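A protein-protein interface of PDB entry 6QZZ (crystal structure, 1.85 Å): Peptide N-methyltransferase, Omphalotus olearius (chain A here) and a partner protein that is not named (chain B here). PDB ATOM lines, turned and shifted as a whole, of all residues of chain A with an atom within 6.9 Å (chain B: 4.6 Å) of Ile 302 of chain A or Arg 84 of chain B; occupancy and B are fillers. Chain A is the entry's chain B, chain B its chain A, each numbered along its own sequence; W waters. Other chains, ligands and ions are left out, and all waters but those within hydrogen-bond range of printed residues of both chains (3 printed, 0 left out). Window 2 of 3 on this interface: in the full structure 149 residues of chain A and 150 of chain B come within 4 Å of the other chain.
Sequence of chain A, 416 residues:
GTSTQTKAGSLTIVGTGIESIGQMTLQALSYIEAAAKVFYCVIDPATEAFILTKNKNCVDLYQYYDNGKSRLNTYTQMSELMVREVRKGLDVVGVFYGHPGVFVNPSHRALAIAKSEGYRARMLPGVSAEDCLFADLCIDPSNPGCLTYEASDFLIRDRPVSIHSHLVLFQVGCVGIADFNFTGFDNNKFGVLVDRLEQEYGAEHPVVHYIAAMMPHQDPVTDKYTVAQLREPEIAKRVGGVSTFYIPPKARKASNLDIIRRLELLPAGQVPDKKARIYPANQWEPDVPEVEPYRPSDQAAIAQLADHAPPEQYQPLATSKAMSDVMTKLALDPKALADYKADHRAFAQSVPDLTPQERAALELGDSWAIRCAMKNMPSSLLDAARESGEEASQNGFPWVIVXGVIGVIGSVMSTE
The side-chain hydroxyl (OG1) of Thr 76 of chain B is in hydrogen-bond range of the side-chain carboxylate (OD1) of Asp 298 of chain A (2.8 Å).
The side-chain carboxylate (OE1) of Glu 80 of chain B is in hydrogen-bond range of the side-chain hydroxyl (OH) of Tyr 294 of chain A (2.6 Å).
NH2 of Arg 87 of chain B lies within hydrogen-bond range of OH of Tyr 294 of chain A.
The side-chain carboxylate (OE2) of Glu 80 of chain B is in salt-bridge range of the guanidinium group (NH1) of Arg 87 of chain B (2.8 Å).
O of Tyr 294 of chain A sits close to OE1 of Gln 299 of chain A (3.3 Å).
Ile 302 of chain A touches Thr 76 of chain B.
Glu 80 of chain B touches Ile 302 of chain A (CD to CD1, 3.7 Å).
Ile 302 of chain A touches Arg 84 of chain B (CG2 to NH2, 3.6 Å).
CD1 of Leu 305 of chain A touches NH1 of Arg 84 of chain B, at 3.8 Å.
Of chain B, only Thr 76, Glu 80 and Arg 84 come within 4 Å of Ile 302 of chain A.
Arg 84 of chain B touches two residues of chain A.
Printed residues of chain B within 4 Å of Asp 298 of chain A: Thr 76.
Printed residues of chain B within 4 Å of Leu 305 of chain A: Arg 84.
Of the printed residues of chain A, Glu 80 of chain B touches Tyr 294 (2.6 Å) and Ile 302 (3.7 Å).
Of the printed residues of chain B, Tyr 294 of chain A touches Glu 80 and Arg 87.
The nearest printed residue of chain B that does not touch Ile 302 of chain A is Arg 87 of chain B (6.8 Å).
Of the 10 printed residues of chain B, 4 touch a printed residue of chain A.
Among the printed residues, no Asp or Glu carboxylate lies within 4 Å of a Lys or Arg side-chain nitrogen of the other chain.
Water W2 lies within hydrogen-bond range of the backbone carbonyl oxygen (O) of Ile 302 of chain A, the guanidinium group (NH2) of Arg 84 of chain B and the backbone NH (N) of Ala 306 of chain A.
Water W1 lies within hydrogen-bond range of NH1 of Arg 84 of chain B and N of Ala 306 of chain A.
Water W3 lies within hydrogen-bond range of OG1 of Thr 76 of chain B and OD1 of Asp 298 of chain A.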
ATOM      1  N   PRO A 293       8.635  26.576 -12.641  1.00  0.00           N
ATOM      2  CA  PRO A 293       8.206  25.893 -13.865  1.00  0.00           C
ATOM      3  C   PRO A 293       7.220  26.700 -14.718  1.00  0.00           C
ATOM      4  O   PRO A 293       7.191  26.503 -15.909  1.00  0.00           O
ATOM      5  CB  PRO A 293       7.522  24.609 -13.361  1.00  0.00           C
ATOM      6  CG  PRO A 293       7.076  24.951 -11.956  1.00  0.00           C
ATOM      7  CD  PRO A 293       8.125  25.912 -11.427  1.00  0.00           C
ATOM      8  N   TYR A 294       6.432  27.596 -14.114  1.00  0.00           N
ATOM      9  CA  TYR A 294       5.421  28.384 -14.857  1.00  0.00           C
ATOM     10  C   TYR A 294       5.710  29.880 -14.729  1.00  0.00           C
ATOM     11  O   TYR A 294       4.969  30.584 -14.031  1.00  0.00           O
ATOM     12  CB  TYR A 294       4.025  27.966 -14.401  1.00  0.00           C
ATOM     13  CG  TYR A 294       3.676  26.558 -14.805  1.00  0.00           C
ATOM     14  CD1 TYR A 294       3.123  26.296 -16.045  1.00  0.00           C
ATOM     15  CD2 TYR A 294       3.927  25.482 -13.969  1.00  0.00           C
ATOM     16  CE1 TYR A 294       2.791  25.011 -16.432  1.00  0.00           C
ATOM     17  CE2 TYR A 294       3.629  24.185 -14.358  1.00  0.00           C
ATOM     18  CZ  TYR A 294       3.047  23.950 -15.587  1.00  0.00           C
ATOM     19  OH  TYR A 294       2.716  22.689 -15.982  1.00  0.00           O
ATOM     20  N   SER A 297       6.402  33.719 -19.387  1.00  0.00           N
ATOM     21  CA  SER A 297       6.694  33.228 -20.763  1.00  0.00           C
ATOM     22  C   SER A 297       6.064  31.838 -20.960  1.00  0.00           C
ATOM     23  O   SER A 297       5.485  31.595 -22.040  1.00  0.00           O
ATOM     24  CB  SER A 297       8.177  33.225 -21.048  1.00  0.00           C
ATOM     25  OG  SER A 297       8.858  32.325 -20.190  1.00  0.00           O
ATOM     26  N   ASP A 298       6.141  30.964 -19.950  1.00  0.00           N
ATOM     27  CA  ASP A 298       5.556  29.591 -19.996  1.00  0.00           C
ATOM     28  C   ASP A 298       4.032  29.695 -20.110  1.00  0.00           C
ATOM     29  O   ASP A 298       3.436  29.054 -21.003  1.00  0.00           O
ATOM     30  CB  ASP A 298       5.961  28.767 -18.773  1.00  0.00           C
ATOM     31  CG  ASP A 298       7.460  28.546 -18.661  1.00  0.00           C
ATOM     32  OD1 ASP A 298       8.031  27.978 -19.608  1.00  0.00           O
ATOM     33  OD2 ASP A 298       8.043  28.955 -17.628  1.00  0.00           O
ATOM     34  N   GLN A 299       3.409  30.508 -19.254  1.00  0.00           N
ATOM     35  CA  GLN A 299       1.933  30.696 -19.231  1.00  0.00           C
ATOM     36  C   GLN A 299       1.452  31.215 -20.597  1.00  0.00           C
ATOM     37  O   GLN A 299       0.471  30.673 -21.116  1.00  0.00           O
ATOM     38  CB  GLN A 299       1.536  31.628 -18.080  1.00  0.00           C
ATOM     39  CG  GLN A 299       1.951  31.100 -16.713  1.00  0.00           C
ATOM     40  CD  GLN A 299       1.683  32.087 -15.603  1.00  0.00           C
ATOM     41  OE1 GLN A 299       2.593  32.693 -15.044  1.00  0.00           O
ATOM     42  NE2 GLN A 299       0.416  32.252 -15.284  1.00  0.00           N
ATOM     43  N   ALA A 300       2.141  32.192 -21.188  1.00  0.00           N
ATOM     44  CA  ALA A 300       1.783  32.748 -22.516  1.00  0.00           C
ATOM     45  C   ALA A 300       1.907  31.667 -23.603  1.00  0.00           C
ATOM     46  O   ALA A 300       1.013  31.587 -24.472  1.00  0.00           O
ATOM     47  CB  ALA A 300       2.638  33.958 -22.818  1.00  0.00           C
ATOM     48  N   ALA A 301       2.956  30.843 -23.577  1.00  0.00           N
ATOM     49  CA  ALA A 301       3.120  29.748 -24.567  1.00  0.00           C
ATOM     50  C   ALA A 301       1.954  28.762 -24.421  1.00  0.00           C
ATOM     51  O   ALA A 301       1.394  28.340 -25.434  1.00  0.00           O
ATOM     52  CB  ALA A 301       4.453  29.080 -24.390  1.00  0.00           C
ATOM     53  N   ILE A 302       1.578  28.415 -23.190  1.00  0.00           N
ATOM     54  CA  ILE A 302       0.469  27.448 -22.920  1.00  0.00           C
ATOM     55  C   ILE A 302      -0.863  28.060 -23.376  1.00  0.00           C
ATOM     56  O   ILE A 302      -1.664  27.326 -23.990  1.00  0.00           O
ATOM     57  CB  ILE A 302       0.488  27.011 -21.440  1.00  0.00           C
ATOM     58  CG1 ILE A 302       1.726  26.150 -21.162  1.00  0.00           C
ATOM     59  CG2 ILE A 302      -0.805  26.306 -21.058  1.00  0.00           C
ATOM     60  CD1 ILE A 302       2.070  26.017 -19.710  1.00  0.00           C
ATOM     61  N   ALA A 303      -1.073  29.363 -23.150  1.00  0.00           N
ATOM     62  CA  ALA A 303      -2.276  30.103 -23.605  1.00  0.00           C
ATOM     63  C   ALA A 303      -2.439  29.976 -25.127  1.00  0.00           C
ATOM     64  O   ALA A 303      -3.589  29.954 -25.587  1.00  0.00           O
ATOM     65  CB  ALA A 303      -2.199  31.548 -23.181  1.00  0.00           C
ATOM     66  N   GLN A 304      -1.340  29.867 -25.880  1.00  0.00           N
ATOM     67  CA  GLN A 304      -1.368  29.797 -27.370  1.00  0.00           C
ATOM     68  C   GLN A 304      -1.885  28.434 -27.852  1.00  0.00           C
ATOM     69  O   GLN A 304      -2.264  28.355 -29.030  1.00  0.00           O
ATOM     70  CB  GLN A 304       0.016  30.071 -27.966  1.00  0.00           C
ATOM     71  CG  GLN A 304       0.462  31.522 -27.854  1.00  0.00           C
ATOM     72  CD  GLN A 304      -0.223  32.409 -28.869  1.00  0.00           C
ATOM     73  OE1 GLN A 304      -1.335  32.140 -29.318  1.00  0.00           O
ATOM     74  NE2 GLN A 304       0.447  33.485 -29.256  1.00  0.00           N
ATOM     75  N   LEU A 305      -1.906  27.400 -27.000  1.00  0.00           N
ATOM     76  CA  LEU A 305      -2.330  26.025 -27.392  1.00  0.00           C
ATOM     77  C   LEU A 305      -3.783  26.005 -27.872  1.00  0.00           C
ATOM     78  O   LEU A 305      -4.096  25.189 -28.759  1.00  0.00           O
ATOM     79  CB  LEU A 305      -2.149  25.053 -26.220  1.00  0.00           C
ATOM     80  CG  LEU A 305      -0.714  24.594 -25.954  1.00  0.00           C
ATOM     81  CD1 LEU A 305      -0.661  23.681 -24.737  1.00  0.00           C
ATOM     82  CD2 LEU A 305      -0.130  23.896 -27.174  1.00  0.00           C
ATOM     83  N   ALA A 306      -4.655  26.839 -27.303  1.00  0.00           N
ATOM     84  CA  ALA A 306      -6.113  26.827 -27.597  1.00  0.00           C
ATOM     85  C   ALA A 306      -6.361  27.042 -29.097  1.00  0.00           C
ATOM     86  O   ALA A 306      -7.204  26.320 -29.678  1.00  0.00           O
ATOM     87  CB  ALA A 306      -6.815  27.887 -26.773  1.00  0.00           C
ATOM     88  N   THR B  76       7.794  24.098 -23.796  1.00  0.00           N
ATOM     89  CA  THR B  76       6.766  24.357 -22.754  1.00  0.00           C
ATOM     90  C   THR B  76       5.436  23.745 -23.218  1.00  0.00           C
ATOM     91  O   THR B  76       4.816  23.011 -22.429  1.00  0.00           O
ATOM     92  CB  THR B  76       6.660  25.844 -22.434  1.00  0.00           C
ATOM     93  OG1 THR B  76       7.866  26.199 -21.761  1.00  0.00           O
ATOM     94  CG2 THR B  76       5.458  26.142 -21.570  1.00  0.00           C
ATOM     95  N   GLU B  80       3.385  20.538 -21.636  1.00  0.00           N
ATOM     96  CA  GLU B  80       2.031  20.808 -21.073  1.00  0.00           C
ATOM     97  C   GLU B  80       1.000  19.864 -21.700  1.00  0.00           C
ATOM     98  O   GLU B  80       0.102  19.418 -20.985  1.00  0.00           O
ATOM     99  CB  GLU B  80       1.631  22.267 -21.252  1.00  0.00           C
ATOM    100  CG  GLU B  80       0.516  22.695 -20.302  1.00  0.00           C
ATOM    101  CD  GLU B  80       0.917  22.652 -18.837  1.00  0.00           C
ATOM    102  OE1 GLU B  80       2.132  22.465 -18.519  1.00  0.00           O
ATOM    103  OE2 GLU B  80       0.011  22.784 -18.005  1.00  0.00           O
ATOM    104  N   LEU B  81       1.127  19.547 -22.985  1.00  0.00           N
ATOM    105  CA  LEU B  81       0.209  18.587 -23.657  1.00  0.00           C
ATOM    106  C   LEU B  81       0.271  17.236 -22.951  1.00  0.00           C
ATOM    107  O   LEU B  81      -0.806  16.624 -22.767  1.00  0.00           O
ATOM    108  CB  LEU B  81       0.591  18.459 -25.128  1.00  0.00           C
ATOM    109  CG  LEU B  81       0.266  19.680 -25.983  1.00  0.00           C
ATOM    110  CD1 LEU B  81       0.917  19.540 -27.330  1.00  0.00           C
ATOM    111  CD2 LEU B  81      -1.244  19.862 -26.131  1.00  0.00           C
ATOM    112  N   MET B  82       1.470  16.786 -22.562  1.00  0.00           N
ATOM    113  CA  MET B  82       1.645  15.473 -21.888  1.00  0.00           C
ATOM    114  C   MET B  82       1.095  15.559 -20.455  1.00  0.00           C
ATOM    115  O   MET B  82       0.282  14.688 -20.061  1.00  0.00           O
ATOM    116  CB  MET B  82       3.103  15.016 -21.866  1.00  0.00           C
ATOM    117  CG  MET B  82       3.633  14.797 -23.263  1.00  0.00           C
ATOM    118  SD  MET B  82       5.265  14.046 -23.264  1.00  0.00           S
ATOM    119  CE  MET B  82       6.265  15.492 -22.931  1.00  0.00           C
ATOM    120  N   VAL B  83       1.464  16.598 -19.717  1.00  0.00           N
ATOM    121  CA  VAL B  83       1.097  16.704 -18.278  1.00  0.00           C
ATOM    122  C   VAL B  83      -0.425  16.926 -18.146  1.00  0.00           C
ATOM    123  O   VAL B  83      -1.001  16.441 -17.153  1.00  0.00           O
ATOM    124  CB  VAL B  83       1.922  17.794 -17.570  1.00  0.00           C
ATOM    125  CG1 VAL B  83       1.354  18.106 -16.203  1.00  0.00           C
ATOM    126  CG2 VAL B  83       3.384  17.367 -17.451  1.00  0.00           C
ATOM    127  N   ARG B  84      -1.055  17.646 -19.065  1.00  0.00           N
ATOM    128  CA  ARG B  84      -2.538  17.816 -19.062  1.00  0.00           C
ATOM    129  C   ARG B  84      -3.227  16.452 -19.007  1.00  0.00           C
ATOM    130  O   ARG B  84      -4.213  16.325 -18.269  1.00  0.00           O
ATOM    131  CB  ARG B  84      -3.019  18.588 -20.282  1.00  0.00           C
ATOM    132  CG  ARG B  84      -2.870  20.089 -20.124  1.00  0.00           C
ATOM    133  CD  ARG B  84      -3.258  20.749 -21.410  1.00  0.00           C
ATOM    134  NE  ARG B  84      -3.307  22.189 -21.273  1.00  0.00           N
ATOM    135  CZ  ARG B  84      -3.665  23.000 -22.258  1.00  0.00           C
ATOM    136  NH1 ARG B  84      -4.017  22.493 -23.425  1.00  0.00           N
ATOM    137  NH2 ARG B  84      -3.685  24.306 -22.070  1.00  0.00           N
ATOM    138  N   GLU B  85      -2.747  15.479 -19.773  1.00  0.00           N
ATOM    139  CA  GLU B  85      -3.361  14.125 -19.864  1.00  0.00           C
ATOM    140  C   GLU B  85      -3.044  13.329 -18.599  1.00  0.00           C
ATOM    141  O   GLU B  85      -3.896  12.521 -18.186  1.00  0.00           O
ATOM    142  CB  GLU B  85      -2.917  13.411 -21.134  1.00  0.00           C
ATOM    143  CG  GLU B  85      -3.299  14.170 -22.389  1.00  0.00           C
ATOM    144  CD  GLU B  85      -4.789  14.422 -22.524  1.00  0.00           C
ATOM    145  OE1 GLU B  85      -5.157  15.537 -22.895  1.00  0.00           O
ATOM    146  OE2 GLU B  85      -5.565  13.515 -22.209  1.00  0.00           O
ATOM    147  N   VAL B  86      -1.886  13.571 -17.985  1.00  0.00           N
ATOM    148  CA  VAL B  86      -1.487  12.928 -16.703  1.00  0.00           C
ATOM    149  C   VAL B  86      -2.484  13.392 -15.637  1.00  0.00           C
ATOM    150  O   VAL B  86      -2.939  12.558 -14.845  1.00  0.00           O
ATOM    151  CB  VAL B  86      -0.035  13.273 -16.308  1.00  0.00           C
ATOM    152  CG1 VAL B  86       0.315  12.751 -14.922  1.00  0.00           C
ATOM    153  CG2 VAL B  86       0.977  12.785 -17.339  1.00  0.00           C
ATOM    154  N   ARG B  87      -2.786  14.685 -15.618  1.00  0.00           N
ATOM    155  CA  ARG B  87      -3.614  15.324 -14.554  1.00  0.00           C
ATOM    156  C   ARG B  87      -5.072  14.845 -14.654  1.00  0.00           C
ATOM    157  O   ARG B  87      -5.763  14.888 -13.632  1.00  0.00           O
ATOM    158  CB  ARG B  87      -3.522  16.846 -14.678  1.00  0.00           C
ATOM    159  CG  ARG B  87      -2.199  17.431 -14.195  1.00  0.00           C
ATOM    160  CD  ARG B  87      -2.050  18.839 -14.738  1.00  0.00           C
ATOM    161  NE  ARG B  87      -0.857  19.535 -14.273  1.00  0.00           N
ATOM    162  CZ  ARG B  87      -0.316  20.591 -14.884  1.00  0.00           C
ATOM    163  NH1 ARG B  87      -0.834  21.061 -16.009  1.00  0.00           N
ATOM    164  NH2 ARG B  87       0.769  21.158 -14.382  1.00  0.00           N
ATOM    165  N   LYS B  88      -5.505  14.408 -15.839  1.00  0.00           N
ATOM    166  CA  LYS B  88      -6.855  13.845 -16.120  1.00  0.00           C
ATOM    167  C   LYS B  88      -6.905  12.356 -15.739  1.00  0.00           C
ATOM    168  O   LYS B  88      -7.977  11.730 -15.947  1.00  0.00           O
ATOM    169  CB  LYS B  88      -7.206  14.057 -17.595  1.00  0.00           C
ATOM    170  CG  LYS B  88      -7.442  15.507 -17.991  1.00  0.00           C
ATOM    171  CD  LYS B  88      -7.416  15.758 -19.492  1.00  0.00           C
ATOM    172  CE  LYS B  88      -8.474  14.998 -20.267  1.00  0.00           C
ATOM    173  NZ  LYS B  88      -8.195  15.002 -21.725  1.00  0.00           N
HETATM  174  O   HOH W   1      -5.567  24.431 -25.171  1.00  0.00           O
HETATM  175  O   HOH W   2      -4.325  26.629 -23.917  1.00  0.00           O
HETATM  176  O   HOH W   3       8.289  29.077 -22.846  1.00  0.00           O
